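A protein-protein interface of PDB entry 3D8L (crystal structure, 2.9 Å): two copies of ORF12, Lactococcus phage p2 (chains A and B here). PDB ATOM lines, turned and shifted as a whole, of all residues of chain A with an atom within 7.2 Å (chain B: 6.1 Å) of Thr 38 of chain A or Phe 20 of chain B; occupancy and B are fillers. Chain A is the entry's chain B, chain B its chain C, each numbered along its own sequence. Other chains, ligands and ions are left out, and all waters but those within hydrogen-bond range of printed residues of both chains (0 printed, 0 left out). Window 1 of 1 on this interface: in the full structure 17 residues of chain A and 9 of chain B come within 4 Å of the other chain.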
ATOM      1  N   GLU A  29     -19.262  20.485   9.337  1.00  0.00           N
ATOM      2  CA  GLU A  29     -20.348  19.695   9.925  1.00  0.00           C
ATOM      3  C   GLU A  29     -20.087  18.191   9.893  1.00  0.00           C
ATOM      4  O   GLU A  29     -20.649  17.433  10.695  1.00  0.00           O
ATOM      5  CB  GLU A  29     -21.649  19.961   9.186  1.00  0.00           C
ATOM      6  CG  GLU A  29     -22.490  21.040   9.828  1.00  0.00           C
ATOM      7  CD  GLU A  29     -22.993  20.626  11.177  1.00  0.00           C
ATOM      8  OE1 GLU A  29     -22.990  19.405  11.436  1.00  0.00           O
ATOM      9  OE2 GLU A  29     -23.383  21.504  11.975  1.00  0.00           O
ATOM     10  N   LEU A  30     -19.259  17.764   8.939  1.00  0.00           N
ATOM     11  CA  LEU A  30     -18.895  16.358   8.777  1.00  0.00           C
ATOM     12  C   LEU A  30     -17.876  15.917   9.813  1.00  0.00           C
ATOM     13  O   LEU A  30     -17.904  14.760  10.240  1.00  0.00           O
ATOM     14  CB  LEU A  30     -18.372  16.085   7.361  1.00  0.00           C
ATOM     15  CG  LEU A  30     -19.427  15.424   6.469  1.00  0.00           C
ATOM     16  CD1 LEU A  30     -19.277  15.838   4.940  1.00  0.00           C
ATOM     17  CD2 LEU A  30     -19.457  13.875   6.727  1.00  0.00           C
ATOM     18  N   GLY A  35     -23.395  16.566  15.140  1.00  0.00           N
ATOM     19  CA  GLY A  35     -23.626  17.357  13.947  1.00  0.00           C
ATOM     20  C   GLY A  35     -24.971  17.098  13.304  1.00  0.00           C
ATOM     21  O   GLY A  35     -25.756  16.231  13.702  1.00  0.00           O
ATOM     22  N   GLU A  36     -25.222  17.874  12.278  1.00  0.00           N
ATOM     23  CA  GLU A  36     -26.505  17.884  11.632  1.00  0.00           C
ATOM     24  C   GLU A  36     -26.301  18.040  10.133  1.00  0.00           C
ATOM     25  O   GLU A  36     -26.973  18.867   9.466  1.00  0.00           O
ATOM     26  CB  GLU A  36     -27.329  19.038  12.184  1.00  0.00           C
ATOM     27  CG  GLU A  36     -28.793  18.835  11.977  1.00  0.00           C
ATOM     28  CD  GLU A  36     -29.598  19.449  13.072  1.00  0.00           C
ATOM     29  OE1 GLU A  36     -29.516  18.972  14.234  1.00  0.00           O
ATOM     30  OE2 GLU A  36     -30.309  20.414  12.760  1.00  0.00           O
ATOM     31  N   ILE A  37     -25.367  17.240   9.609  1.00  0.00           N
ATOM     32  CA  ILE A  37     -25.032  17.363   8.211  1.00  0.00           C
ATOM     33  C   ILE A  37     -26.268  17.111   7.374  1.00  0.00           C
ATOM     34  O   ILE A  37     -26.455  17.801   6.395  1.00  0.00           O
ATOM     35  CB  ILE A  37     -23.856  16.492   7.785  1.00  0.00           C
ATOM     36  CG1 ILE A  37     -23.728  16.585   6.267  1.00  0.00           C
ATOM     37  CG2 ILE A  37     -24.026  15.087   8.281  1.00  0.00           C
ATOM     38  CD1 ILE A  37     -22.372  16.377   5.760  1.00  0.00           C
ATOM     39  N   THR A  38     -27.128  16.171   7.779  1.00  0.00           N
ATOM     40  CA  THR A  38     -28.362  15.882   7.036  1.00  0.00           C
ATOM     41  C   THR A  38     -29.107  17.153   6.712  1.00  0.00           C
ATOM     42  O   THR A  38     -29.347  17.437   5.545  1.00  0.00           O
ATOM     43  CB  THR A  38     -29.335  14.973   7.782  1.00  0.00           C
ATOM     44  OG1 THR A  38     -28.715  13.711   8.031  1.00  0.00           O
ATOM     45  CG2 THR A  38     -30.588  14.754   6.953  1.00  0.00           C
ATOM     46  N   ASP A  39     -29.456  17.930   7.732  1.00  0.00           N
ATOM     47  CA  ASP A  39     -30.238  19.156   7.526  1.00  0.00           C
ATOM     48  C   ASP A  39     -29.504  20.205   6.695  1.00  0.00           C
ATOM     49  O   ASP A  39     -30.138  20.943   5.955  1.00  0.00           O
ATOM     50  CB  ASP A  39     -30.618  19.787   8.861  1.00  0.00           C
ATOM     51  CG  ASP A  39     -31.444  21.071   8.701  1.00  0.00           C
ATOM     52  OD1 ASP A  39     -32.495  21.016   8.038  1.00  0.00           O
ATOM     53  OD2 ASP A  39     -31.046  22.125   9.244  1.00  0.00           O
ATOM     54  N   LEU A  40     -28.177  20.277   6.836  1.00  0.00           N
ATOM     55  CA  LEU A  40     -27.353  21.246   6.098  1.00  0.00           C
ATOM     56  C   LEU A  40     -27.334  20.866   4.648  1.00  0.00           C
ATOM     57  O   LEU A  40     -27.486  21.715   3.788  1.00  0.00           O
ATOM     58  CB  LEU A  40     -25.905  21.268   6.604  1.00  0.00           C
ATOM     59  CG  LEU A  40     -25.186  22.624   6.615  1.00  0.00           C
ATOM     60  CD1 LEU A  40     -23.667  22.441   6.551  1.00  0.00           C
ATOM     61  CD2 LEU A  40     -25.649  23.529   5.507  1.00  0.00           C
ATOM     62  N   MET A  41     -27.139  19.587   4.375  1.00  0.00           N
ATOM     63  CA  MET A  41     -27.092  19.131   3.001  1.00  0.00           C
ATOM     64  C   MET A  41     -28.412  19.372   2.275  1.00  0.00           C
ATOM     65  O   MET A  41     -28.394  19.738   1.109  1.00  0.00           O
ATOM     66  CB  MET A  41     -26.717  17.657   2.923  1.00  0.00           C
ATOM     67  CG  MET A  41     -25.242  17.390   2.807  1.00  0.00           C
ATOM     68  SD  MET A  41     -25.166  15.637   2.658  1.00  0.00           S
ATOM     69  CE  MET A  41     -23.391  15.395   2.825  1.00  0.00           C
ATOM     70  N   GLU A  42     -29.540  19.177   2.960  1.00  0.00           N
ATOM     71  CA  GLU A  42     -30.852  19.281   2.328  1.00  0.00           C
ATOM     72  C   GLU A  42     -31.204  20.746   2.166  1.00  0.00           C
ATOM     73  O   GLU A  42     -31.874  21.138   1.199  1.00  0.00           O
ATOM     74  CB  GLU A  42     -31.900  18.514   3.142  1.00  0.00           C
ATOM     75  CG  GLU A  42     -31.592  17.006   3.163  1.00  0.00           C
ATOM     76  CD  GLU A  42     -32.662  16.104   3.770  1.00  0.00           C
ATOM     77  OE1 GLU A  42     -33.808  16.549   3.964  1.00  0.00           O
ATOM     78  OE2 GLU A  42     -32.342  14.917   4.040  1.00  0.00           O
ATOM     79  N   PHE A  43     -30.729  21.558   3.112  1.00  0.00           N
ATOM     80  CA  PHE A  43     -30.799  23.012   3.032  1.00  0.00           C
ATOM     81  C   PHE A  43     -30.128  23.439   1.747  1.00  0.00           C
ATOM     82  O   PHE A  43     -30.749  24.086   0.914  1.00  0.00           O
ATOM     83  CB  PHE A  43     -30.071  23.636   4.210  1.00  0.00           C
ATOM     84  CG  PHE A  43     -30.311  25.090   4.377  1.00  0.00           C
ATOM     85  CD1 PHE A  43     -31.240  25.553   5.309  1.00  0.00           C
ATOM     86  CD2 PHE A  43     -29.584  26.015   3.670  1.00  0.00           C
ATOM     87  CE1 PHE A  43     -31.445  26.893   5.509  1.00  0.00           C
ATOM     88  CE2 PHE A  43     -29.805  27.397   3.870  1.00  0.00           C
ATOM     89  CZ  PHE A  43     -30.729  27.817   4.781  1.00  0.00           C
ATOM     90  N   VAL A  44     -28.862  23.070   1.565  1.00  0.00           N
ATOM     91  CA  VAL A  44     -28.138  23.554   0.413  1.00  0.00           C
ATOM     92  C   VAL A  44     -28.778  22.946  -0.818  1.00  0.00           C
ATOM     93  O   VAL A  44     -28.986  23.641  -1.815  1.00  0.00           O
ATOM     94  CB  VAL A  44     -26.639  23.232   0.461  1.00  0.00           C
ATOM     95  CG1 VAL A  44     -25.988  23.654  -0.808  1.00  0.00           C
ATOM     96  CG2 VAL A  44     -25.967  23.930   1.604  1.00  0.00           C
ATOM     97  N   GLN A  45     -29.147  21.669  -0.747  1.00  0.00           N
ATOM     98  CA  GLN A  45     -29.704  20.990  -1.916  1.00  0.00           C
ATOM     99  C   GLN A  45     -30.939  21.679  -2.433  1.00  0.00           C
ATOM    100  O   GLN A  45     -31.070  21.840  -3.622  1.00  0.00           O
ATOM    101  CB  GLN A  45     -30.050  19.524  -1.635  1.00  0.00           C
ATOM    102  CG  GLN A  45     -30.572  18.784  -2.877  1.00  0.00           C
ATOM    103  CD  GLN A  45     -30.911  17.326  -2.640  1.00  0.00           C
ATOM    104  OE1 GLN A  45     -31.136  16.584  -3.572  1.00  0.00           O
ATOM    105  NE2 GLN A  45     -30.955  16.920  -1.395  1.00  0.00           N
ATOM    106  N   PHE A  67     -40.568  24.285   3.522  1.00  0.00           N
ATOM    107  CA  PHE A  67     -39.654  23.197   3.780  1.00  0.00           C
ATOM    108  C   PHE A  67     -38.911  23.399   5.106  1.00  0.00           C
ATOM    109  O   PHE A  67     -38.612  22.421   5.789  1.00  0.00           O
ATOM    110  CB  PHE A  67     -38.680  23.048   2.605  1.00  0.00           C
ATOM    111  CG  PHE A  67     -37.301  22.582   2.992  1.00  0.00           C
ATOM    112  CD1 PHE A  67     -37.007  21.231   3.107  1.00  0.00           C
ATOM    113  CD2 PHE A  67     -36.291  23.495   3.221  1.00  0.00           C
ATOM    114  CE1 PHE A  67     -35.728  20.810   3.453  1.00  0.00           C
ATOM    115  CE2 PHE A  67     -35.017  23.068   3.572  1.00  0.00           C
ATOM    116  CZ  PHE A  67     -34.734  21.737   3.684  1.00  0.00           C
ATOM    117  N   SER B   6     -36.997  12.980   3.114  1.00  0.00           N
ATOM    118  CA  SER B   6     -35.908  12.169   2.573  1.00  0.00           C
ATOM    119  C   SER B   6     -35.694  10.945   3.423  1.00  0.00           C
ATOM    120  O   SER B   6     -36.024  10.939   4.607  1.00  0.00           O
ATOM    121  CB  SER B   6     -34.603  12.954   2.533  1.00  0.00           C
ATOM    122  OG  SER B   6     -34.072  13.176   3.825  1.00  0.00           O
ATOM    123  N   ALA B   8     -32.893   9.818   4.578  1.00  0.00           N
ATOM    124  CA  ALA B   8     -31.945  10.205   5.645  1.00  0.00           C
ATOM    125  C   ALA B   8     -32.576  10.981   6.804  1.00  0.00           C
ATOM    126  O   ALA B   8     -32.059  10.930   7.912  1.00  0.00           O
ATOM    127  CB  ALA B   8     -30.787  10.997   5.076  1.00  0.00           C
ATOM    128  N   ARG B   9     -33.656  11.716   6.546  1.00  0.00           N
ATOM    129  CA  ARG B   9     -34.453  12.315   7.621  1.00  0.00           C
ATOM    130  C   ARG B   9     -35.120  11.222   8.416  1.00  0.00           C
ATOM    131  O   ARG B   9     -35.156  11.233   9.644  1.00  0.00           O
ATOM    132  CB  ARG B   9     -35.575  13.217   7.080  1.00  0.00           C
ATOM    133  CG  ARG B   9     -35.350  14.735   7.141  1.00  0.00           C
ATOM    134  CD  ARG B   9     -34.472  15.131   8.333  1.00  0.00           C
ATOM    135  NE  ARG B   9     -34.571  16.533   8.729  1.00  0.00           N
ATOM    136  CZ  ARG B   9     -34.201  17.578   7.999  1.00  0.00           C
ATOM    137  NH1 ARG B   9     -33.738  17.446   6.768  1.00  0.00           N
ATOM    138  NH2 ARG B   9     -34.322  18.788   8.518  1.00  0.00           N
ATOM    139  N   LYS B  12     -32.791   9.510  10.829  1.00  0.00           N
ATOM    140  CA  LYS B  12     -32.487  10.261  12.051  1.00  0.00           C
ATOM    141  C   LYS B  12     -33.668  10.175  12.994  1.00  0.00           C
ATOM    142  O   LYS B  12     -33.497  10.077  14.211  1.00  0.00           O
ATOM    143  CB  LYS B  12     -32.144  11.735  11.771  1.00  0.00           C
ATOM    144  CG  LYS B  12     -31.248  12.413  12.849  1.00  0.00           C
ATOM    145  CD  LYS B  12     -31.244  13.945  12.641  1.00  0.00           C
ATOM    146  CE  LYS B  12     -29.962  14.715  13.123  1.00  0.00           C
ATOM    147  NZ  LYS B  12     -29.600  14.438  14.553  1.00  0.00           N
ATOM    148  N   ASP B  18     -27.303  10.501  12.703  1.00  0.00           N
ATOM    149  CA  ASP B  18     -27.207  11.074  11.379  1.00  0.00           C
ATOM    150  C   ASP B  18     -26.466  10.141  10.406  1.00  0.00           C
ATOM    151  O   ASP B  18     -25.242   9.932  10.511  1.00  0.00           O
ATOM    152  CB  ASP B  18     -26.533  12.431  11.442  1.00  0.00           C
ATOM    153  CG  ASP B  18     -26.746  13.221  10.197  1.00  0.00           C
ATOM    154  OD1 ASP B  18     -26.438  12.663   9.129  1.00  0.00           O
ATOM    155  OD2 ASP B  18     -27.223  14.387  10.285  1.00  0.00           O
ATOM    156  N   LEU B  19     -27.257   9.611   9.463  1.00  0.00           N
ATOM    157  CA  LEU B  19     -26.846   8.685   8.418  1.00  0.00           C
ATOM    158  C   LEU B  19     -25.545   9.066   7.743  1.00  0.00           C
ATOM    159  O   LEU B  19     -24.697   8.215   7.481  1.00  0.00           O
ATOM    160  CB  LEU B  19     -27.940   8.647   7.357  1.00  0.00           C
ATOM    161  CG  LEU B  19     -28.188   7.384   6.550  1.00  0.00           C
ATOM    162  CD1 LEU B  19     -29.009   7.740   5.339  1.00  0.00           C
ATOM    163  CD2 LEU B  19     -26.907   6.768   6.136  1.00  0.00           C
ATOM    164  N   PHE B  20     -25.373  10.337   7.444  1.00  0.00           N
ATOM    165  CA  PHE B  20     -24.161  10.723   6.771  1.00  0.00           C
ATOM    166  C   PHE B  20     -22.985  10.614   7.710  1.00  0.00           C
ATOM    167  O   PHE B  20     -21.952  10.104   7.321  1.00  0.00           O
ATOM    168  CB  PHE B  20     -24.272  12.113   6.181  1.00  0.00           C
ATOM    169  CG  PHE B  20     -25.254  12.203   5.059  1.00  0.00           C
ATOM    170  CD1 PHE B  20     -26.600  12.446   5.315  1.00  0.00           C
ATOM    171  CD2 PHE B  20     -24.841  12.037   3.749  1.00  0.00           C
ATOM    172  CE1 PHE B  20     -27.511  12.533   4.284  1.00  0.00           C
ATOM    173  CE2 PHE B  20     -25.746  12.118   2.709  1.00  0.00           C
ATOM    174  CZ  PHE B  20     -27.083  12.370   2.977  1.00  0.00           C
ATOM    175  N   GLN B  21     -23.139  11.058   8.951  1.00  0.00           N
ATOM    176  CA  GLN B  21     -22.068  10.883   9.934  1.00  0.00           C
ATOM    177  C   GLN B  21     -21.691   9.412  10.049  1.00  0.00           C
ATOM    178  O   GLN B  21     -20.509   9.047  10.016  1.00  0.00           O
ATOM    179  CB  GLN B  21     -22.465  11.459  11.302  1.00  0.00           C
ATOM    180  CG  GLN B  21     -21.994  12.912  11.478  1.00  0.00           C
ATOM    181  CD  GLN B  21     -22.867  13.784  12.404  1.00  0.00           C
ATOM    182  OE1 GLN B  21     -22.836  15.022  12.321  1.00  0.00           O
ATOM    183  NE2 GLN B  21     -23.634  13.147  13.282  1.00  0.00           N
ATOM    184  N   GLN B  22     -22.717   8.574  10.111  1.00  0.00           N
ATOM    185  CA  GLN B  22     -22.553   7.168  10.439  1.00  0.00           C
ATOM    186  C   GLN B  22     -21.751   6.332   9.464  1.00  0.00           C
ATOM    187  O   GLN B  22     -21.393   5.240   9.821  1.00  0.00           O
ATOM    188  CB  GLN B  22     -23.906   6.530  10.656  1.00  0.00           C
ATOM    189  CG  GLN B  22     -24.559   7.014  11.926  1.00  0.00           C
ATOM    190  CD  GLN B  22     -24.139   6.202  13.129  1.00  0.00           C
ATOM    191  OE1 GLN B  22     -23.661   6.716  14.136  1.00  0.00           O
ATOM    192  NE2 GLN B  22     -24.329   4.913  13.026  1.00  0.00           N
ATOM    193  N   GLN B  23     -21.453   6.797   8.258  1.00  0.00           N
ATOM    194  CA  GLN B  23     -20.529   6.034   7.422  1.00  0.00           C
ATOM    195  C   GLN B  23     -19.106   6.494   7.584  1.00  0.00           C
ATOM    196  O   GLN B  23     -18.170   5.710   7.416  1.00  0.00           O
ATOM    197  CB  GLN B  23     -20.879   6.162   5.975  1.00  0.00           C
ATOM    198  CG  GLN B  23     -22.064   5.350   5.566  1.00  0.00           C
ATOM    199  CD  GLN B  23     -22.778   6.050   4.454  1.00  0.00           C
ATOM    200  OE1 GLN B  23     -22.572   5.737   3.267  1.00  0.00           O
ATOM    201  NE2 GLN B  23     -23.558   7.083   4.818  1.00  0.00           N
ATOM    202  N   LYS B  24     -18.928   7.779   7.861  1.00  0.00           N
ATOM    203  CA  LYS B  24     -17.623   8.232   8.288  1.00  0.00           C
ATOM    204  C   LYS B  24     -17.218   7.458   9.537  1.00  0.00           C
ATOM    205  O   LYS B  24     -16.057   7.064   9.676  1.00  0.00           O
ATOM    206  CB  LYS B  24     -17.607   9.734   8.535  1.00  0.00           C
ATOM    207  CG  LYS B  24     -17.151  10.491   7.322  1.00  0.00           C
ATOM    208  CD  LYS B  24     -16.653  11.862   7.690  1.00  0.00           C
ATOM    209  CE  LYS B  24     -16.254  12.628   6.446  1.00  0.00           C
ATOM    210  NZ  LYS B  24     -15.910  14.037   6.740  1.00  0.00           N
ATOM    211  N   ALA B  25     -18.181   7.223  10.425  1.00  0.00           N
ATOM    212  CA  ALA B  25     -17.942   6.417  11.610  1.00  0.00           C
ATOM    213  C   ALA B  25     -17.461   5.020  11.210  1.00  0.00           C
ATOM    214  O   ALA B  25     -16.413   4.576  11.706  1.00  0.00           O
ATOM    215  CB  ALA B  25     -19.184   6.342  12.448  1.00  0.00           C
ATOM    216  N   TRP B  87     -30.351   3.685  -1.273  1.00  0.00           N
ATOM    217  CA  TRP B  87     -30.308   5.017  -0.724  1.00  0.00           C
ATOM    218  C   TRP B  87     -29.541   5.970  -1.632  1.00  0.00           C
ATOM    219  O   TRP B  87     -30.042   7.022  -1.952  1.00  0.00           O
ATOM    220  CB  TRP B  87     -29.680   4.982   0.663  1.00  0.00           C
ATOM    221  CG  TRP B  87     -29.436   6.336   1.211  1.00  0.00           C
ATOM    222  CD1 TRP B  87     -30.322   7.343   1.283  1.00  0.00           C
ATOM    223  CD2 TRP B  87     -28.219   6.827   1.761  1.00  0.00           C
ATOM    224  NE1 TRP B  87     -29.742   8.446   1.832  1.00  0.00           N
ATOM    225  CE2 TRP B  87     -28.444   8.157   2.133  1.00  0.00           C
ATOM    226  CE3 TRP B  87     -26.959   6.270   1.976  1.00  0.00           C
ATOM    227  CZ2 TRP B  87     -27.459   8.951   2.707  1.00  0.00           C
ATOM    228  CZ3 TRP B  87     -25.976   7.055   2.544  1.00  0.00           C
ATOM    229  CH2 TRP B  87     -26.231   8.382   2.907  1.00  0.00           C
ATOM    230  N   ILE B  91     -29.321  10.819  -4.269  1.00  0.00           N
ATOM    231  CA  ILE B  91     -28.094  11.530  -3.795  1.00  0.00           C
ATOM    232  C   ILE B  91     -27.289  12.235  -4.935  1.00  0.00           C
ATOM    233  O   ILE B  91     -26.867  13.397  -4.837  1.00  0.00           O
ATOM    234  CB  ILE B  91     -27.149  10.565  -2.935  1.00  0.00           C
ATOM    235  CG1 ILE B  91     -27.108  10.990  -1.435  1.00  0.00           C
ATOM    236  CG2 ILE B  91     -25.720  10.461  -3.544  1.00  0.00           C
ATOM    237  CD1 ILE B  91     -26.564  12.429  -1.179  1.00  0.00           C
ATOM    238  OXT ILE B  91     -27.018  11.685  -6.006  1.00  0.00           O
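Glu 29 of chain A touches Gln 21 of chain B (O to OE1, 3.6 Å).
Leu 30 of chain A touches Lys 24 of chain B.
OD2 of Asp 18 of chain B touches C of Glu 36 of chain A, at 3.8 Å.
Gln 21 of chain B touches Glu 36 of chain A.
CB of Phe 20 of chain B touches CG2 of Ile 37 of chain A, 3.6 Å away.
Thr 38 of chain A touches Phe 20 of chain B (OG1 to CD1, 3.7 Å).
Phe 20 of chain B touches Met 41 of chain A.
OE1 of Glu 29 of chain A sits at hydrogen-bond distance from N of Glu 36 of chain A.
The backbone NH (N) of Arg 9 of chain B lies within hydrogen-bond range of the side-chain hydroxyl (OG) of Ser 6 of chain B, at 3.1 Å.
The side-chain carboxylate (OD1) of Asp 18 of chain B lies within hydrogen-bond range of the backbone NH (N) of Phe 20 of chain B (3.1 Å).
N of Gly 35 of chain A sits close to OE1 of Gln 21 of chain B.
The backbone NH of Ile 37 of chain A lies within hydrogen-bond range of the side-chain carboxylate of Asp 18 of chain B.
OG1 of Thr 38 of chain A lies within hydrogen-bond range of OD1 of Asp 18 of chain B.
The side-chain carboxylate of Asp 39 of chain A is in salt-bridge range of the guanidinium group of Arg 9 of chain B, 2.9 Å away.
The side-chain carboxylate (OE2) of Glu 42 of chain A is in hydrogen-bond range of the side-chain hydroxyl (OG) of Ser 6 of chain B, 2.5 Å away.
The guanidinium group (NH1) of Arg 9 of chain B lies within salt-bridge range of the side-chain carboxylate (OE1) of Glu 42 of chain A (2.9 Å).
Of the printed residues of chain B, Leu 30 of chain A touches Lys 24.
Printed residues of chain B within 4 Å of Asp 39 of chain A: Arg 9 (2.9 Å).
Gln 45 of chain A touches none of the printed residues of chain B.
Phe 20 of chain B touches three residues of chain A.
The nearest residue of chain B that does not touch Thr 38 of chain A is Arg 9 of chain B (4.1 Å).
No position is printed for both chains.
Of the 13 pairs that touch across the chains among the printed residues, none has its exchanged pair printed and touching as well.
Hydrophobic or aromatic side chains of chain A that line the printed part of chain B: Leu 30, Ile 37 and Met 41.
Along chain A the printed residues that touch a printed residue of chain B span positions 29 to 42.
Of the 14 printed residues of chain B, 6 touch a printed residue of chain A.
Among the printed residues, 13 pairs touch across the chains.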
